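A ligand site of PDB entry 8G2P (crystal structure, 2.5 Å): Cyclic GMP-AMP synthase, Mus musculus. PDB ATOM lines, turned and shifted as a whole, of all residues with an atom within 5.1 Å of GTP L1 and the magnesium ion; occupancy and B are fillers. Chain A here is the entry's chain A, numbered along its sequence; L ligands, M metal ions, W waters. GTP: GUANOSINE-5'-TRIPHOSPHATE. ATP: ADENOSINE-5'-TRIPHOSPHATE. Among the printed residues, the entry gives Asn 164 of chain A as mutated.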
ATOM      1  N   THR A  54      27.039  -6.993  26.614  1.00  0.00           N
ATOM      2  CA  THR A  54      26.061  -6.718  25.557  1.00  0.00           C
ATOM      3  C   THR A  54      24.771  -6.101  26.078  1.00  0.00           C
ATOM      4  O   THR A  54      24.578  -5.897  27.274  1.00  0.00           O
ATOM      5  CB  THR A  54      25.747  -7.997  24.790  1.00  0.00           C
ATOM      6  OG1 THR A  54      25.480  -8.988  25.761  1.00  0.00           O
ATOM      7  CG2 THR A  54      26.912  -8.389  23.913  1.00  0.00           C
ATOM      8  N   GLY A  55      23.916  -5.728  25.135  1.00  0.00           N
ATOM      9  CA  GLY A  55      22.627  -5.159  25.494  1.00  0.00           C
ATOM     10  C   GLY A  55      22.734  -3.681  25.844  1.00  0.00           C
ATOM     11  O   GLY A  55      23.783  -3.057  25.652  1.00  0.00           O
ATOM     12  N   SER A  56      21.653  -3.151  26.397  1.00  0.00           N
ATOM     13  CA  SER A  56      21.394  -1.732  26.387  1.00  0.00           C
ATOM     14  C   SER A  56      22.422  -0.959  27.194  1.00  0.00           C
ATOM     15  O   SER A  56      22.836   0.128  26.761  1.00  0.00           O
ATOM     16  CB  SER A  56      19.992  -1.430  26.852  1.00  0.00           C
ATOM     17  OG  SER A  56      19.717  -2.072  28.095  1.00  0.00           O
ATOM     18  N   GLU A  68      19.798  -3.201  35.040  1.00  0.00           N
ATOM     19  CA  GLU A  68      19.703  -4.429  34.273  1.00  0.00           C
ATOM     20  C   GLU A  68      20.896  -4.489  33.325  1.00  0.00           C
ATOM     21  O   GLU A  68      21.081  -3.614  32.494  1.00  0.00           O
ATOM     22  CB  GLU A  68      18.326  -4.518  33.592  1.00  0.00           C
ATOM     23  CG  GLU A  68      17.844  -5.930  33.264  1.00  0.00           C
ATOM     24  CD  GLU A  68      18.063  -6.498  31.864  1.00  0.00           C
ATOM     25  OE1 GLU A  68      19.016  -6.111  31.154  1.00  0.00           O
ATOM     26  OE2 GLU A  68      17.237  -7.343  31.470  1.00  0.00           O
ATOM     27  N   ASP A  70      23.394  -7.174  30.813  1.00  0.00           N
ATOM     28  CA  ASP A  70      23.413  -8.445  30.113  1.00  0.00           C
ATOM     29  C   ASP A  70      24.850  -8.816  29.771  1.00  0.00           C
ATOM     30  O   ASP A  70      25.523  -8.067  29.077  1.00  0.00           O
ATOM     31  CB  ASP A  70      22.515  -8.389  28.877  1.00  0.00           C
ATOM     32  CG  ASP A  70      21.152  -7.789  29.169  1.00  0.00           C
ATOM     33  OD1 ASP A  70      20.366  -8.407  29.928  1.00  0.00           O
ATOM     34  OD2 ASP A  70      20.884  -6.703  28.646  1.00  0.00           O
ATOM     35  N   MET A  72      27.357 -11.970  28.274  1.00  0.00           N
ATOM     36  CA  MET A  72      27.458 -13.263  27.598  1.00  0.00           C
ATOM     37  C   MET A  72      28.738 -13.917  28.094  1.00  0.00           C
ATOM     38  O   MET A  72      29.774 -13.283  28.156  1.00  0.00           O
ATOM     39  CB  MET A  72      27.485 -13.068  26.070  1.00  0.00           C
ATOM     40  CG  MET A  72      26.163 -13.361  25.365  1.00  0.00           C
ATOM     41  SD  MET A  72      26.079 -13.100  23.540  1.00  0.00           S
ATOM     42  CE  MET A  72      26.414 -11.366  23.640  1.00  0.00           C
ATOM     43  N   LYS A 145      13.142 -19.250  34.508  1.00  0.00           N
ATOM     44  CA  LYS A 145      12.052 -19.174  33.534  1.00  0.00           C
ATOM     45  C   LYS A 145      12.303 -20.224  32.468  1.00  0.00           C
ATOM     46  O   LYS A 145      13.348 -20.163  31.831  1.00  0.00           O
ATOM     47  CB  LYS A 145      11.978 -17.783  32.895  1.00  0.00           C
ATOM     48  CG  LYS A 145      12.010 -16.665  33.934  1.00  0.00           C
ATOM     49  CD  LYS A 145      11.518 -15.313  33.475  1.00  0.00           C
ATOM     50  CE  LYS A 145      11.119 -14.452  34.660  1.00  0.00           C
ATOM     51  NZ  LYS A 145      10.155 -13.395  34.285  1.00  0.00           N
ATOM     52  N   PRO A 146      11.408 -21.236  32.275  1.00  0.00           N
ATOM     53  CA  PRO A 146      11.650 -22.285  31.272  1.00  0.00           C
ATOM     54  C   PRO A 146      11.869 -21.719  29.866  1.00  0.00           C
ATOM     55  O   PRO A 146      11.300 -20.675  29.515  1.00  0.00           O
ATOM     56  CB  PRO A 146      10.387 -23.175  31.335  1.00  0.00           C
ATOM     57  CG  PRO A 146       9.824 -22.900  32.727  1.00  0.00           C
ATOM     58  CD  PRO A 146      10.182 -21.458  33.053  1.00  0.00           C
ATOM     59  N   GLY A 147      12.772 -22.359  29.105  1.00  0.00           N
ATOM     60  CA  GLY A 147      13.179 -21.908  27.783  1.00  0.00           C
ATOM     61  C   GLY A 147      13.949 -20.572  27.725  1.00  0.00           C
ATOM     62  O   GLY A 147      14.257 -20.117  26.636  1.00  0.00           O
ATOM     63  N   SER A 148      14.271 -19.933  28.866  1.00  0.00           N
ATOM     64  CA  SER A 148      15.157 -18.753  28.886  1.00  0.00           C
ATOM     65  C   SER A 148      16.628 -19.151  28.840  1.00  0.00           C
ATOM     66  O   SER A 148      17.094 -20.071  29.525  1.00  0.00           O
ATOM     67  CB  SER A 148      14.918 -17.860  30.091  1.00  0.00           C
ATOM     68  OG  SER A 148      15.903 -16.835  30.191  1.00  0.00           O
ATOM     69  N   PRO A 149      17.458 -18.424  28.072  1.00  0.00           N
ATOM     70  CA  PRO A 149      18.883 -18.742  27.987  1.00  0.00           C
ATOM     71  C   PRO A 149      19.684 -18.222  29.192  1.00  0.00           C
ATOM     72  O   PRO A 149      20.877 -18.480  29.296  1.00  0.00           O
ATOM     73  CB  PRO A 149      19.283 -18.007  26.700  1.00  0.00           C
ATOM     74  CG  PRO A 149      18.404 -16.750  26.766  1.00  0.00           C
ATOM     75  CD  PRO A 149      17.072 -17.233  27.287  1.00  0.00           C
ATOM     76  N   ALA A 150      19.033 -17.464  30.084  1.00  0.00           N
ATOM     77  CA  ALA A 150      19.750 -16.678  31.071  1.00  0.00           C
ATOM     78  C   ALA A 150      19.760 -17.371  32.436  1.00  0.00           C
ATOM     79  O   ALA A 150      18.791 -17.989  32.827  1.00  0.00           O
ATOM     80  CB  ALA A 150      19.130 -15.318  31.205  1.00  0.00           C
ATOM     81  N   ASN A 164      21.870 -10.653  33.880  1.00  0.00           N
ATOM     82  CA  ASN A 164      21.568 -11.828  33.088  1.00  0.00           C
ATOM     83  C   ASN A 164      22.875 -12.399  32.556  1.00  0.00           C
ATOM     84  O   ASN A 164      23.527 -11.763  31.736  1.00  0.00           O
ATOM     85  CB  ASN A 164      20.623 -11.453  31.950  1.00  0.00           C
ATOM     86  CG  ASN A 164      19.339 -10.817  32.447  1.00  0.00           C
ATOM     87  OD1 ASN A 164      19.069  -9.661  32.150  1.00  0.00           O
ATOM     88  ND2 ASN A 164      18.559 -11.551  33.209  1.00  0.00           N
ATOM     89  N   ILE A 166      24.355 -14.953  30.214  1.00  0.00           N
ATOM     90  CA  ILE A 166      23.907 -15.728  29.067  1.00  0.00           C
ATOM     91  C   ILE A 166      25.045 -16.626  28.555  1.00  0.00           C
ATOM     92  O   ILE A 166      26.001 -16.143  27.988  1.00  0.00           O
ATOM     93  CB  ILE A 166      23.375 -14.783  27.979  1.00  0.00           C
ATOM     94  CG1 ILE A 166      22.292 -13.871  28.539  1.00  0.00           C
ATOM     95  CG2 ILE A 166      22.868 -15.549  26.777  1.00  0.00           C
ATOM     96  CD1 ILE A 166      22.735 -12.461  28.745  1.00  0.00           C
ATOM     97  N   VAL A 205      22.628 -19.402  21.716  1.00  0.00           N
ATOM     98  CA  VAL A 205      22.228 -19.414  23.108  1.00  0.00           C
ATOM     99  C   VAL A 205      21.132 -20.436  23.281  1.00  0.00           C
ATOM    100  O   VAL A 205      20.431 -20.737  22.338  1.00  0.00           O
ATOM    101  CB  VAL A 205      21.814 -18.020  23.570  1.00  0.00           C
ATOM    102  CG1 VAL A 205      22.948 -17.043  23.368  1.00  0.00           C
ATOM    103  CG2 VAL A 205      20.533 -17.545  22.902  1.00  0.00           C
ATOM    104  N   ARG A 221      19.415 -20.969  19.817  1.00  0.00           N
ATOM    105  CA  ARG A 221      18.973 -19.794  19.074  1.00  0.00           C
ATOM    106  C   ARG A 221      20.198 -18.912  18.777  1.00  0.00           C
ATOM    107  O   ARG A 221      21.080 -18.745  19.633  1.00  0.00           O
ATOM    108  CB  ARG A 221      17.917 -19.036  19.883  1.00  0.00           C
ATOM    109  CG  ARG A 221      17.285 -17.842  19.153  1.00  0.00           C
ATOM    110  CD  ARG A 221      16.302 -16.998  19.971  1.00  0.00           C
ATOM    111  NE  ARG A 221      16.959 -16.128  20.946  1.00  0.00           N
ATOM    112  CZ  ARG A 221      16.384 -15.641  22.053  1.00  0.00           C
ATOM    113  NH1 ARG A 221      15.094 -15.813  22.275  1.00  0.00           N
ATOM    114  NH2 ARG A 221      17.097 -14.942  22.917  1.00  0.00           N
ATOM    115  N   LEU A 222      20.237 -18.343  17.562  1.00  0.00           N
ATOM    116  CA  LEU A 222      21.306 -17.438  17.169  1.00  0.00           C
ATOM    117  C   LEU A 222      21.233 -16.148  17.974  1.00  0.00           C
ATOM    118  O   LEU A 222      20.142 -15.693  18.308  1.00  0.00           O
ATOM    119  CB  LEU A 222      21.220 -17.117  15.674  1.00  0.00           C
ATOM    120  CG  LEU A 222      21.604 -18.280  14.766  1.00  0.00           C
ATOM    121  CD1 LEU A 222      21.066 -18.111  13.363  1.00  0.00           C
ATOM    122  CD2 LEU A 222      23.100 -18.455  14.748  1.00  0.00           C
ATOM    123  N   SER A 223      22.402 -15.588  18.290  1.00  0.00           N
ATOM    124  CA  SER A 223      22.498 -14.255  18.855  1.00  0.00           C
ATOM    125  C   SER A 223      23.481 -13.427  18.022  1.00  0.00           C
ATOM    126  O   SER A 223      24.540 -13.932  17.589  1.00  0.00           O
ATOM    127  CB  SER A 223      22.942 -14.286  20.286  1.00  0.00           C
ATOM    128  OG  SER A 223      23.207 -12.970  20.771  1.00  0.00           O
ATOM    129  N   PHE A 224      23.116 -12.156  17.859  1.00  0.00           N
ATOM    130  CA  PHE A 224      23.899 -11.175  17.122  1.00  0.00           C
ATOM    131  C   PHE A 224      24.154  -9.943  17.981  1.00  0.00           C
ATOM    132  O   PHE A 224      24.395  -8.856  17.481  1.00  0.00           O
ATOM    133  CB  PHE A 224      23.144 -10.828  15.836  1.00  0.00           C
ATOM    134  CG  PHE A 224      23.060 -11.991  14.904  1.00  0.00           C
ATOM    135  CD1 PHE A 224      24.180 -12.420  14.215  1.00  0.00           C
ATOM    136  CD2 PHE A 224      21.898 -12.729  14.796  1.00  0.00           C
ATOM    137  CE1 PHE A 224      24.126 -13.517  13.388  1.00  0.00           C
ATOM    138  CE2 PHE A 224      21.840 -13.847  13.959  1.00  0.00           C
ATOM    139  CZ  PHE A 224      22.948 -14.232  13.268  1.00  0.00           C
ATOM    140  N   SER A 225      24.111 -10.147  19.297  1.00  0.00           N
ATOM    141  CA  SER A 225      24.238  -9.078  20.270  1.00  0.00           C
ATOM    142  C   SER A 225      25.520  -8.293  20.065  1.00  0.00           C
ATOM    143  O   SER A 225      25.545  -7.106  20.291  1.00  0.00           O
ATOM    144  CB  SER A 225      24.176  -9.638  21.653  1.00  0.00           C
ATOM    145  OG  SER A 225      22.887 -10.164  21.919  1.00  0.00           O
HETATM  146  PG  GTP L   1      10.391 -14.993  25.709  1.00  0.00           P
HETATM  147  O1G GTP L   1      10.707 -13.482  26.138  1.00  0.00           O
HETATM  148  O2G GTP L   1      10.594 -15.310  24.174  1.00  0.00           O
HETATM  149  O3G GTP L   1       9.052 -15.520  26.326  1.00  0.00           O
HETATM  150  O3B GTP L   1      11.448 -16.010  26.398  1.00  0.00           O
HETATM  151  PB  GTP L   1      12.345 -15.820  27.713  1.00  0.00           P
HETATM  152  O1B GTP L   1      11.854 -14.553  28.410  1.00  0.00           O
HETATM  153  O2B GTP L   1      12.380 -17.158  28.448  1.00  0.00           O
HETATM  154  O3A GTP L   1      13.750 -15.579  26.932  1.00  0.00           O
HETATM  155  PA  GTP L   1      14.267 -14.223  26.217  1.00  0.00           P
HETATM  156  O1A GTP L   1      14.395 -14.509  24.739  1.00  0.00           O
HETATM  157  O2A GTP L   1      13.363 -13.145  26.747  1.00  0.00           O
HETATM  158  O5' GTP L   1      15.732 -14.046  26.893  1.00  0.00           O
HETATM  159  C5' GTP L   1      15.755 -13.736  28.317  1.00  0.00           C
HETATM  160  C4' GTP L   1      16.746 -12.638  28.612  1.00  0.00           C
HETATM  161  O4' GTP L   1      18.100 -13.140  28.411  1.00  0.00           O
HETATM  162  C3' GTP L   1      16.688 -11.395  27.712  1.00  0.00           C
HETATM  163  O3' GTP L   1      15.770 -10.452  28.238  1.00  0.00           O
HETATM  164  C2' GTP L   1      18.104 -10.863  27.875  1.00  0.00           C
HETATM  165  O2' GTP L   1      18.267 -10.302  29.154  1.00  0.00           O
HETATM  166  C1' GTP L   1      18.879 -12.165  27.741  1.00  0.00           C
HETATM  167  N9  GTP L   1      19.120 -12.612  26.363  1.00  0.00           N
HETATM  168  C8  GTP L   1      18.351 -13.426  25.561  1.00  0.00           C
HETATM  169  N7  GTP L   1      18.901 -13.659  24.382  1.00  0.00           N
HETATM  170  C5  GTP L   1      20.110 -12.973  24.410  1.00  0.00           C
HETATM  171  C6  GTP L   1      21.125 -12.837  23.414  1.00  0.00           C
HETATM  172  O6  GTP L   1      21.133 -13.298  22.261  1.00  0.00           O
HETATM  173  N1  GTP L   1      22.189 -12.031  23.868  1.00  0.00           N
HETATM  174  C2  GTP L   1      22.223 -11.386  25.100  1.00  0.00           C
HETATM  175  N2  GTP L   1      23.290 -10.608  25.379  1.00  0.00           N
HETATM  176  N3  GTP L   1      21.268 -11.532  26.026  1.00  0.00           N
HETATM  177  C4  GTP L   1      20.255 -12.323  25.629  1.00  0.00           C
HETATM  178  PG  ATP L   2      16.704  -3.512  27.838  1.00  0.00           P
HETATM  179  O1G ATP L   2      15.198  -3.678  27.697  1.00  0.00           O
HETATM  180  O2G ATP L   2      17.046  -2.141  28.397  1.00  0.00           O
HETATM  181  O3G ATP L   2      17.280  -4.654  28.712  1.00  0.00           O
HETATM  182  PB  ATP L   2      18.338  -4.835  25.756  1.00  0.00           P
HETATM  183  O1B ATP L   2      18.700  -4.770  24.289  1.00  0.00           O
HETATM  184  O2B ATP L   2      19.478  -5.054  26.726  1.00  0.00           O
HETATM  185  O3B ATP L   2      17.372  -3.661  26.294  1.00  0.00           O
HETATM  186  PA  ATP L   2      17.325  -7.462  26.704  1.00  0.00           P
HETATM  187  O1A ATP L   2      15.945  -8.046  26.740  1.00  0.00           O
HETATM  188  O2A ATP L   2      18.102  -7.148  27.958  1.00  0.00           O
HETATM  189  O3A ATP L   2      17.273  -6.046  25.935  1.00  0.00           O
HETATM  190  O5' ATP L   2      18.194  -8.401  25.741  1.00  0.00           O
HETATM  191  C5' ATP L   2      19.643  -8.277  25.712  1.00  0.00           C
HETATM  192  C4' ATP L   2      20.115  -8.550  24.296  1.00  0.00           C
HETATM  193  O4' ATP L   2      19.779  -9.917  23.910  1.00  0.00           O
HETATM  194  C3' ATP L   2      19.505  -7.654  23.199  1.00  0.00           C
HETATM  195  O3' ATP L   2      20.293  -6.468  23.042  1.00  0.00           O
HETATM  196  C2' ATP L   2      19.628  -8.543  21.957  1.00  0.00           C
HETATM  197  O2' ATP L   2      20.922  -8.371  21.440  1.00  0.00           O
HETATM  198  C1' ATP L   2      19.433  -9.956  22.542  1.00  0.00           C
HETATM  199  N9  ATP L   2      18.065 -10.457  22.444  1.00  0.00           N
HETATM  200  C8  ATP L   2      17.019 -10.235  23.346  1.00  0.00           C
HETATM  201  N7  ATP L   2      15.917 -10.841  22.959  1.00  0.00           N
HETATM  202  C5  ATP L   2      16.254 -11.479  21.769  1.00  0.00           C
HETATM  203  C6  ATP L   2      15.500 -12.251  20.852  1.00  0.00           C
HETATM  204  N6  ATP L   2      14.217 -12.537  21.031  1.00  0.00           N
HETATM  205  N1  ATP L   2      16.136 -12.731  19.753  1.00  0.00           N
HETATM  206  C2  ATP L   2      17.424 -12.398  19.556  1.00  0.00           C
HETATM  207  N3  ATP L   2      18.224 -11.675  20.347  1.00  0.00           N
HETATM  208  C4  ATP L   2      17.568 -11.245  21.433  1.00  0.00           C
HETATM  209 MG    MG M   1      19.189  -5.180  28.790  1.00  0.00          MG
HETATM  210  O   HOH W   1      20.862  -3.877  29.808  1.00  0.00           O
HETATM  211  O   HOH W   2      19.084 -14.654  20.933  1.00  0.00           O
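Water W1 bridges O of Glu 68 (2.7 Å) and OG of Ser 56 (2.7 Å).
An oxygen (O3') of GTP L1 sits at hydrogen-bond distance from an oxygen (O1A) of ATP L2.
The side-chain carboxylate (OD1) of Asp 70 is in hydrogen-bond range of an oxygen (O2') of GTP L1, at 2.9 Å. O6 of GTP L1 is in hydrogen-bond range of OG of Ser 223, at 2.6 Å. The guanidinium group of Arg 221 is in salt-bridge range of an oxygen (O1A) of GTP L1, at 2.9 Å. OG1 of Thr 54 sits at hydrogen-bond distance from N2 of GTP L1. N1 of GTP L1 lies within hydrogen-bond range of OG of Ser 225, at 2.8 Å. An oxygen (O2B) of GTP L1 lies close to the backbone NH (N) of Ser 148, at 3.4 Å. O2' of GTP L1 is in hydrogen-bond range of OD1 of Asn 164 (3.2 Å). An oxygen (O2') of ATP L2 is in hydrogen-bond range of the side-chain hydroxyl (OG) of Ser 225, at 2.7 Å. An oxygen (O2B) of ATP L2 lies close to the backbone NH (N) of Ser 56, 2.9 Å away. The side-chain hydroxyl (OG) of Ser 56 lies within hydrogen-bond range of an oxygen (O2G) of ATP L2 (2.7 Å).
The magnesium ion is bound by O3G of ATP L2, O2B of ATP L2, OD2 of Asp 70, water W1, O2A of ATP L2 and OE1 of Glu 68. The magnesium ion has six donor atoms within binding distance.
The backbone carbonyl oxygen (O) of Asp 70 sits at hydrogen-bond distance from the backbone NH (N) of Thr 54 (3.1 Å). The side-chain amide oxygen of Asn 164 sits close to the side-chain carboxylate of Asp 70, 2.9 Å away. The side-chain amide oxygen (OD1) of Asn 164 sits close to the side-chain carboxylate (OE2) of Glu 68 (3.0 Å). OG of Ser 225 is in hydrogen-bond range of OG of Ser 223. The backbone carbonyl oxygen (O) of Arg 221 lies within hydrogen-bond range of the backbone NH (N) of Val 205, at 2.7 Å. OG of Ser 148 lies close to N of Ala 150, 3.2 Å away.
Merely in contact with the magnesium ion: Ser 56 (3.2 Å). The nearest printed residue that does not touch the magnesium ion is Gly 55 (4.8 Å).
CE of Met 72 touches N2 of GTP L1, at 3.7 Å. Pro 146 touches GTP L1. C of Gly 147 touches O2B of GTP L1, at 3.8 Å. CD of Pro 149 touches O5' of GTP L1, 3.5 Å away. CB of Ala 150 touches O4' of GTP L1, 3.7 Å away. Ile 166 touches GTP L1 (CD1 to N3, 3.2 Å). Hydrophobic or aromatic side chains that line GTP L1: Met 72, Pro 149, Ala 150 and Ile 166. 14 residues have an atom within 4 Å of GTP L1: Thr 54, Glu 68, Asp 70, Met 72, Pro 146, Gly 147, Ser 148, Pro 149, Ala 150, Asn 164, Ile 166, Arg 221, Ser 223 and Ser 225.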
